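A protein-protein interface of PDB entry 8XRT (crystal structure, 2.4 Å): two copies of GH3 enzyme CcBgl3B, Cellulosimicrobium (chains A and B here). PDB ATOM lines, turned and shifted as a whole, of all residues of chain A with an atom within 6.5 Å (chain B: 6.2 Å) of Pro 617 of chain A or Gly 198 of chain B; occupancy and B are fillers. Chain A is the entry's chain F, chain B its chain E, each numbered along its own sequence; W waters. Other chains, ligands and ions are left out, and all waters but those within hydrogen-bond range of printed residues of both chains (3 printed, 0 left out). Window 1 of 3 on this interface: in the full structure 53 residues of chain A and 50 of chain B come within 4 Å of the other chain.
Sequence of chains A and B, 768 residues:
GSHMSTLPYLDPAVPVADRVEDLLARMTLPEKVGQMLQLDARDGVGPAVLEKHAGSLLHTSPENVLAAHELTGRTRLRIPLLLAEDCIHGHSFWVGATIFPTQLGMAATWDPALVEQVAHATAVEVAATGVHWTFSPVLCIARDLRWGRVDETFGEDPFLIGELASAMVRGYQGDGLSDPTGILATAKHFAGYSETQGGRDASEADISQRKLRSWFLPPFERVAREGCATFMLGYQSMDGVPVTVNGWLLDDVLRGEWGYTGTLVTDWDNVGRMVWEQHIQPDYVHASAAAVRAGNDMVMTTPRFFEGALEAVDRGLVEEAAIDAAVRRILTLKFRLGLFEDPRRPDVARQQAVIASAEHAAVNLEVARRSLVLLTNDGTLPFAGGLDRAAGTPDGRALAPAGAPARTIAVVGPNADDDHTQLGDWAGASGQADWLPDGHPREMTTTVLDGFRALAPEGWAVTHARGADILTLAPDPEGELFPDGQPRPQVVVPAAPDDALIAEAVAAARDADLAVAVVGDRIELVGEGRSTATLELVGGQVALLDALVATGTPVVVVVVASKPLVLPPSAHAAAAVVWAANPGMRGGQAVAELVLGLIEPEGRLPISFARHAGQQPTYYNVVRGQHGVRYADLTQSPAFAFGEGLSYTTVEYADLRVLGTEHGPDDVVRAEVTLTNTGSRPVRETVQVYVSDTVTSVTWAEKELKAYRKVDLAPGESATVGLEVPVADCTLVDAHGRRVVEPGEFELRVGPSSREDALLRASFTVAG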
ATOM      1  N   ARG A 143      10.264 -16.234   0.687  1.00  0.00           N
ATOM      2  CA  ARG A 143      10.996 -17.343   0.086  1.00  0.00           C
ATOM      3  C   ARG A 143      10.963 -17.374  -1.449  1.00  0.00           C
ATOM      4  O   ARG A 143      11.806 -18.047  -2.046  1.00  0.00           O
ATOM      5  CB  ARG A 143      10.462 -18.678   0.611  1.00  0.00           C
ATOM      6  CG  ARG A 143      10.420 -18.745   2.131  1.00  0.00           C
ATOM      7  CD  ARG A 143      11.487 -19.626   2.675  1.00  0.00           C
ATOM      8  NE  ARG A 143      11.278 -21.028   2.316  1.00  0.00           N
ATOM      9  CZ  ARG A 143      12.152 -22.011   2.577  1.00  0.00           C
ATOM     10  NH1 ARG A 143      13.288 -21.746   3.230  1.00  0.00           N
ATOM     11  NH2 ARG A 143      11.882 -23.262   2.203  1.00  0.00           N
ATOM     12  N   ALA A 613      15.509 -14.758 -12.193  1.00  0.00           N
ATOM     13  CA  ALA A 613      14.408 -15.458 -11.530  1.00  0.00           C
ATOM     14  C   ALA A 613      14.641 -16.965 -11.511  1.00  0.00           C
ATOM     15  O   ALA A 613      14.291 -17.647 -10.536  1.00  0.00           O
ATOM     16  CB  ALA A 613      13.064 -15.121 -12.193  1.00  0.00           C
ATOM     17  N   GLY A 614      15.259 -17.499 -12.560  1.00  0.00           N
ATOM     18  CA  GLY A 614      15.567 -18.923 -12.616  1.00  0.00           C
ATOM     19  C   GLY A 614      16.693 -19.352 -11.692  1.00  0.00           C
ATOM     20  O   GLY A 614      16.939 -20.558 -11.552  1.00  0.00           O
ATOM     21  N   GLN A 615      17.348 -18.397 -11.028  1.00  0.00           N
ATOM     22  CA  GLN A 615      18.365 -18.728 -10.045  1.00  0.00           C
ATOM     23  C   GLN A 615      17.783 -19.214  -8.729  1.00  0.00           C
ATOM     24  O   GLN A 615      18.527 -19.760  -7.912  1.00  0.00           O
ATOM     25  CB  GLN A 615      19.255 -17.505  -9.788  1.00  0.00           C
ATOM     26  CG  GLN A 615      20.576 -17.818  -9.181  1.00  0.00           C
ATOM     27  CD  GLN A 615      21.299 -16.572  -8.779  1.00  0.00           C
ATOM     28  OE1 GLN A 615      20.673 -15.532  -8.508  1.00  0.00           O
ATOM     29  NE2 GLN A 615      22.617 -16.642  -8.772  1.00  0.00           N
ATOM     30  N   GLN A 616      16.486 -19.034  -8.508  1.00  0.00           N
ATOM     31  CA  GLN A 616      15.901 -19.256  -7.192  1.00  0.00           C
ATOM     32  C   GLN A 616      15.883 -20.749  -6.851  1.00  0.00           C
ATOM     33  O   GLN A 616      15.776 -21.588  -7.741  1.00  0.00           O
ATOM     34  CB  GLN A 616      14.480 -18.689  -7.141  1.00  0.00           C
ATOM     35  CG  GLN A 616      14.444 -17.181  -7.247  1.00  0.00           C
ATOM     36  CD  GLN A 616      13.114 -16.599  -6.793  1.00  0.00           C
ATOM     37  OE1 GLN A 616      12.978 -16.122  -5.657  1.00  0.00           O
ATOM     38  NE2 GLN A 616      12.115 -16.641  -7.682  1.00  0.00           N
ATOM     39  N   PRO A 617      15.932 -21.105  -5.561  1.00  0.00           N
ATOM     40  CA  PRO A 617      15.959 -20.208  -4.401  1.00  0.00           C
ATOM     41  C   PRO A 617      17.308 -19.543  -4.163  1.00  0.00           C
ATOM     42  O   PRO A 617      18.381 -20.162  -4.242  1.00  0.00           O
ATOM     43  CB  PRO A 617      15.611 -21.141  -3.237  1.00  0.00           C
ATOM     44  CG  PRO A 617      15.983 -22.476  -3.699  1.00  0.00           C
ATOM     45  CD  PRO A 617      15.675 -22.497  -5.155  1.00  0.00           C
ATOM     46  N   THR A 618      17.258 -18.258  -3.833  1.00  0.00           N
ATOM     47  CA  THR A 618      18.471 -17.541  -3.467  1.00  0.00           C
ATOM     48  C   THR A 618      18.502 -17.122  -1.991  1.00  0.00           C
ATOM     49  O   THR A 618      19.374 -16.329  -1.627  1.00  0.00           O
ATOM     50  CB  THR A 618      18.640 -16.314  -4.378  1.00  0.00           C
ATOM     51  OG1 THR A 618      17.424 -15.560  -4.394  1.00  0.00           O
ATOM     52  CG2 THR A 618      18.968 -16.749  -5.831  1.00  0.00           C
ATOM     53  N   TYR A 619      17.566 -17.595  -1.138  1.00  0.00           N
ATOM     54  CA  TYR A 619      17.683 -17.280   0.296  1.00  0.00           C
ATOM     55  C   TYR A 619      18.888 -18.033   0.890  1.00  0.00           C
ATOM     56  O   TYR A 619      19.344 -19.042   0.346  1.00  0.00           O
ATOM     57  CB  TYR A 619      16.379 -17.589   1.066  1.00  0.00           C
ATOM     58  CG  TYR A 619      15.754 -18.920   0.743  1.00  0.00           C
ATOM     59  CD1 TYR A 619      16.266 -20.095   1.283  1.00  0.00           C
ATOM     60  CD2 TYR A 619      14.653 -19.012  -0.116  1.00  0.00           C
ATOM     61  CE1 TYR A 619      15.726 -21.332   0.968  1.00  0.00           C
ATOM     62  CE2 TYR A 619      14.090 -20.263  -0.434  1.00  0.00           C
ATOM     63  CZ  TYR A 619      14.652 -21.416   0.109  1.00  0.00           C
ATOM     64  OH  TYR A 619      14.136 -22.651  -0.180  1.00  0.00           O
ATOM     65  N   VAL A 622      19.718 -22.413   2.516  1.00  0.00           N
ATOM     66  CA  VAL A 622      19.304 -23.469   1.590  1.00  0.00           C
ATOM     67  C   VAL A 622      19.582 -24.845   2.186  1.00  0.00           C
ATOM     68  O   VAL A 622      20.652 -25.101   2.753  1.00  0.00           O
ATOM     69  CB  VAL A 622      20.019 -23.300   0.232  1.00  0.00           C
ATOM     70  CG1 VAL A 622      19.540 -24.360  -0.750  1.00  0.00           C
ATOM     71  CG2 VAL A 622      19.724 -21.946  -0.336  1.00  0.00           C
ATOM     72  N   TYR A 631      24.436 -23.519 -11.850  1.00  0.00           N
ATOM     73  CA  TYR A 631      23.743 -23.873 -13.077  1.00  0.00           C
ATOM     74  C   TYR A 631      24.757 -23.859 -14.217  1.00  0.00           C
ATOM     75  O   TYR A 631      25.808 -23.213 -14.137  1.00  0.00           O
ATOM     76  CB  TYR A 631      22.589 -22.902 -13.350  1.00  0.00           C
ATOM     77  CG  TYR A 631      21.458 -22.934 -12.306  1.00  0.00           C
ATOM     78  CD1 TYR A 631      21.499 -22.120 -11.186  1.00  0.00           C
ATOM     79  CD2 TYR A 631      20.350 -23.782 -12.461  1.00  0.00           C
ATOM     80  CE1 TYR A 631      20.466 -22.131 -10.240  1.00  0.00           C
ATOM     81  CE2 TYR A 631      19.322 -23.800 -11.544  1.00  0.00           C
ATOM     82  CZ  TYR A 631      19.397 -22.983 -10.413  1.00  0.00           C
ATOM     83  OH  TYR A 631      18.384 -22.989  -9.476  1.00  0.00           O
ATOM     84  N   GLN A 636      25.178 -19.925  -8.869  1.00  0.00           N
ATOM     85  CA  GLN A 636      24.136 -19.889  -7.837  1.00  0.00           C
ATOM     86  C   GLN A 636      24.364 -18.788  -6.801  1.00  0.00           C
ATOM     87  O   GLN A 636      23.471 -18.513  -5.989  1.00  0.00           O
ATOM     88  CB  GLN A 636      24.008 -21.257  -7.153  1.00  0.00           C
ATOM     89  CG  GLN A 636      23.080 -22.150  -7.918  1.00  0.00           C
ATOM     90  CD  GLN A 636      23.173 -23.604  -7.573  1.00  0.00           C
ATOM     91  OE1 GLN A 636      23.200 -24.447  -8.472  1.00  0.00           O
ATOM     92  NE2 GLN A 636      23.200 -23.925  -6.287  1.00  0.00           N
ATOM     93  N   ASP B 144       9.821 -29.087 -13.888  1.00  0.00           N
ATOM     94  CA  ASP B 144      10.620 -27.861 -13.867  1.00  0.00           C
ATOM     95  C   ASP B 144      11.606 -27.921 -15.037  1.00  0.00           C
ATOM     96  O   ASP B 144      12.435 -28.832 -15.089  1.00  0.00           O
ATOM     97  CB  ASP B 144      11.362 -27.722 -12.534  1.00  0.00           C
ATOM     98  CG  ASP B 144      11.885 -26.315 -12.288  1.00  0.00           C
ATOM     99  OD1 ASP B 144      12.296 -25.652 -13.269  1.00  0.00           O
ATOM    100  OD2 ASP B 144      11.932 -25.877 -11.098  1.00  0.00           O
ATOM    101  N   ARG B 146      14.092 -26.053 -15.794  1.00  0.00           N
ATOM    102  CA  ARG B 146      15.471 -25.811 -15.414  1.00  0.00           C
ATOM    103  C   ARG B 146      16.235 -27.111 -15.181  1.00  0.00           C
ATOM    104  O   ARG B 146      17.460 -27.134 -15.325  1.00  0.00           O
ATOM    105  CB  ARG B 146      15.503 -24.939 -14.164  1.00  0.00           C
ATOM    106  CG  ARG B 146      15.070 -23.509 -14.391  1.00  0.00           C
ATOM    107  CD  ARG B 146      15.054 -22.739 -13.063  1.00  0.00           C
ATOM    108  NE  ARG B 146      14.162 -23.377 -12.089  1.00  0.00           N
ATOM    109  CZ  ARG B 146      13.931 -22.959 -10.835  1.00  0.00           C
ATOM    110  NH1 ARG B 146      13.093 -23.647 -10.083  1.00  0.00           N
ATOM    111  NH2 ARG B 146      14.515 -21.873 -10.347  1.00  0.00           N
ATOM    112  N   TRP B 147      15.542 -28.191 -14.845  1.00  0.00           N
ATOM    113  CA  TRP B 147      16.214 -29.455 -14.583  1.00  0.00           C
ATOM    114  C   TRP B 147      17.033 -29.930 -15.781  1.00  0.00           C
ATOM    115  O   TRP B 147      16.568 -29.911 -16.929  1.00  0.00           O
ATOM    116  CB  TRP B 147      15.172 -30.496 -14.228  1.00  0.00           C
ATOM    117  CG  TRP B 147      15.680 -31.653 -13.487  1.00  0.00           C
ATOM    118  CD1 TRP B 147      16.526 -31.638 -12.409  1.00  0.00           C
ATOM    119  CD2 TRP B 147      15.326 -33.023 -13.717  1.00  0.00           C
ATOM    120  NE1 TRP B 147      16.756 -32.934 -11.987  1.00  0.00           N
ATOM    121  CE2 TRP B 147      16.023 -33.799 -12.757  1.00  0.00           C
ATOM    122  CE3 TRP B 147      14.517 -33.675 -14.670  1.00  0.00           C
ATOM    123  CZ2 TRP B 147      15.923 -35.194 -12.704  1.00  0.00           C
ATOM    124  CZ3 TRP B 147      14.424 -35.053 -14.637  1.00  0.00           C
ATOM    125  CH2 TRP B 147      15.105 -35.805 -13.633  1.00  0.00           C
ATOM    126  N   THR B 196      12.688 -30.803  -7.817  1.00  0.00           N
ATOM    127  CA  THR B 196      13.441 -30.444  -6.624  1.00  0.00           C
ATOM    128  C   THR B 196      13.729 -28.944  -6.644  1.00  0.00           C
ATOM    129  O   THR B 196      13.566 -28.283  -7.670  1.00  0.00           O
ATOM    130  CB  THR B 196      14.752 -31.246  -6.528  1.00  0.00           C
ATOM    131  OG1 THR B 196      15.525 -31.052  -7.719  1.00  0.00           O
ATOM    132  CG2 THR B 196      14.470 -32.750  -6.330  1.00  0.00           C
ATOM    133  N   GLN B 197      14.134 -28.409  -5.492  1.00  0.00           N
ATOM    134  CA  GLN B 197      14.400 -26.980  -5.338  1.00  0.00           C
ATOM    135  C   GLN B 197      15.249 -26.424  -6.471  1.00  0.00           C
ATOM    136  O   GLN B 197      16.360 -26.910  -6.736  1.00  0.00           O
ATOM    137  CB  GLN B 197      15.126 -26.718  -4.011  1.00  0.00           C
ATOM    138  CG  GLN B 197      14.393 -27.196  -2.769  1.00  0.00           C
ATOM    139  CD  GLN B 197      14.837 -26.462  -1.515  1.00  0.00           C
ATOM    140  OE1 GLN B 197      15.967 -25.966  -1.431  1.00  0.00           O
ATOM    141  NE2 GLN B 197      13.950 -26.408  -0.516  1.00  0.00           N
ATOM    142  N   GLY B 198      14.742 -25.367  -7.097  1.00  0.00           N
ATOM    143  CA  GLY B 198      15.501 -24.610  -8.070  1.00  0.00           C
ATOM    144  C   GLY B 198      15.738 -25.309  -9.389  1.00  0.00           C
ATOM    145  O   GLY B 198      16.537 -24.825 -10.190  1.00  0.00           O
ATOM    146  N   GLY B 199      15.077 -26.434  -9.646  1.00  0.00           N
ATOM    147  CA  GLY B 199      15.456 -27.232 -10.798  1.00  0.00           C
ATOM    148  C   GLY B 199      16.840 -27.843 -10.706  1.00  0.00           C
ATOM    149  O   GLY B 199      17.342 -28.350 -11.705  1.00  0.00           O
ATOM    150  N   ARG B 200      17.455 -27.847  -9.528  1.00  0.00           N
ATOM    151  CA  ARG B 200      18.813 -28.337  -9.378  1.00  0.00           C
ATOM    152  C   ARG B 200      18.844 -29.857  -9.289  1.00  0.00           C
ATOM    153  O   ARG B 200      17.828 -30.513  -9.047  1.00  0.00           O
ATOM    154  CB  ARG B 200      19.446 -27.724  -8.147  1.00  0.00           C
ATOM    155  CG  ARG B 200      19.567 -26.240  -8.297  1.00  0.00           C
ATOM    156  CD  ARG B 200      19.646 -25.554  -6.975  1.00  0.00           C
ATOM    157  NE  ARG B 200      19.364 -24.143  -7.146  1.00  0.00           N
ATOM    158  CZ  ARG B 200      19.440 -23.239  -6.180  1.00  0.00           C
ATOM    159  NH1 ARG B 200      19.807 -23.609  -4.959  1.00  0.00           N
ATOM    160  NH2 ARG B 200      19.156 -21.974  -6.445  1.00  0.00           N
ATOM    161  N   SER B 203      18.849 -31.647  -5.443  1.00  0.00           N
ATOM    162  CA  SER B 203      18.543 -30.808  -4.308  1.00  0.00           C
ATOM    163  C   SER B 203      17.320 -31.390  -3.585  1.00  0.00           C
ATOM    164  O   SER B 203      16.818 -32.462  -3.917  1.00  0.00           O
ATOM    165  CB  SER B 203      18.318 -29.370  -4.772  1.00  0.00           C
ATOM    166  OG  SER B 203      17.328 -29.334  -5.806  1.00  0.00           O
ATOM    167  N   SER B 531      21.849 -28.479 -14.574  1.00  0.00           N
ATOM    168  CA  SER B 531      20.625 -27.702 -14.683  1.00  0.00           C
ATOM    169  C   SER B 531      20.952 -26.308 -15.207  1.00  0.00           C
ATOM    170  O   SER B 531      22.082 -25.825 -15.088  1.00  0.00           O
ATOM    171  CB  SER B 531      19.931 -27.604 -13.319  1.00  0.00           C
ATOM    172  OG  SER B 531      19.698 -28.898 -12.778  1.00  0.00           O
ATOM    173  N   THR B 532      19.954 -25.646 -15.788  1.00  0.00           N
ATOM    174  CA  THR B 532      20.138 -24.290 -16.294  1.00  0.00           C
ATOM    175  C   THR B 532      19.130 -23.366 -15.632  1.00  0.00           C
ATOM    176  O   THR B 532      18.008 -23.776 -15.337  1.00  0.00           O
ATOM    177  CB  THR B 532      19.982 -24.202 -17.843  1.00  0.00           C
ATOM    178  OG1 THR B 532      18.730 -24.782 -18.256  1.00  0.00           O
ATOM    179  CG2 THR B 532      21.146 -24.900 -18.599  1.00  0.00           C
HETATM  180  O   HOH W   1      16.072 -24.886   0.865  1.00  0.00           O
HETATM  181  O   HOH W   2      21.514 -21.475  -3.592  1.00  0.00           O
HETATM  182  O   HOH W   3      13.892 -24.918   2.314  1.00  0.00           O
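The guanidinium group (NH2) of Arg 146 of chain B is in hydrogen-bond range of the backbone carbonyl oxygen (O) of Gly 614 of chain A, at 3.0 Å. The backbone carbonyl oxygen of Gln 616 of chain A is in hydrogen-bond range of the guanidinium group of Arg 146 of chain B, at 2.9 Å. OH of Tyr 631 of chain A lies within hydrogen-bond range of O of Gly 198 of chain B (2.7 Å). The backbone carbonyl oxygen (O) of Gln 615 of chain A sits at hydrogen-bond distance from the guanidinium group (NH2) of Arg 200 of chain B (2.7 Å). O of Pro 617 of chain A lies within hydrogen-bond range of NH2 of Arg 200 of chain B. The guanidinium group (NE) of Arg 200 of chain B lies within hydrogen-bond range of the side-chain hydroxyl (OH) of Tyr 631 of chain A (2.8 Å).
The side-chain carboxylate of Asp 144 of chain B lies within salt-bridge range of the guanidinium group of Arg 146 of chain B (2.7 Å). O of Arg 146 of chain B is in hydrogen-bond range of N of Thr 532 of chain B. The backbone carbonyl oxygen (O) of Arg 200 of chain B is in hydrogen-bond range of the side-chain hydroxyl (OG1) of Thr 196 of chain B, 2.7 Å away. The backbone carbonyl oxygen (O) of Gln 197 of chain B lies within hydrogen-bond range of the side-chain hydroxyl (OG) of Ser 203 of chain B. NE2 of Gln 615 of chain A sits close to O of Gln 636 of chain A (3.5 Å). OH of Tyr 631 of chain A sits at hydrogen-bond distance from O of Gln 616 of chain A (3.4 Å).
Gln 616 of chain A touches Gly 198 of chain B (O to CA, 3.1 Å). Arg 200 of chain B touches Gln 616 of chain A (NH2 to C, 3.5 Å). Pro 617 of chain A touches Gly 198 of chain B. Tyr 619 of chain A touches Gln 197 of chain B. CG1 of Val 622 of chain A touches OE1 of Gln 197 of chain B, 3.98 Å away. CA of Tyr 631 of chain A touches O of Ser 531 of chain B, 3.3 Å away. Thr 532 of chain B touches Tyr 631 of chain A. Gln 636 of chain A touches Arg 200 of chain B.
Gly 198 of chain B touches three residues of chain A. Of the printed residues of chain A, Thr 532 of chain B touches Tyr 631. Of the printed residues of chain A, Ser 531 of chain B touches Tyr 631. The nearest residue of chain A that does not touch Gly 198 of chain B is Gly 614 of chain A (4.5 Å).
Of the 11 printed residues of chain B, 6 touch a printed residue of chain A. Along chain B the printed residues that touch a printed residue of chain A span positions 146 to 532. Hydrophobic or aromatic side chains of chain A that line the printed part of chain B: Pro 617, Tyr 619, Val 622 and Tyr 631.
No position is printed for both chains.
Water W1 lies within hydrogen-bond range of the side-chain amide oxygen of Gln 197 of chain B (2.5 Å) and the side-chain hydroxyl of Tyr 619 of chain A (3.1 Å). Water W3 lies within hydrogen-bond range of NH2 of Arg 143 of chain A (2.6 Å), NE2 of Gln 197 of chain B (3.2 Å) and OH of Tyr 619 of chain A (3.4 Å). Water W2 bridges NH1 of Arg 200 of chain B and O of Pro 617 of chain A.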
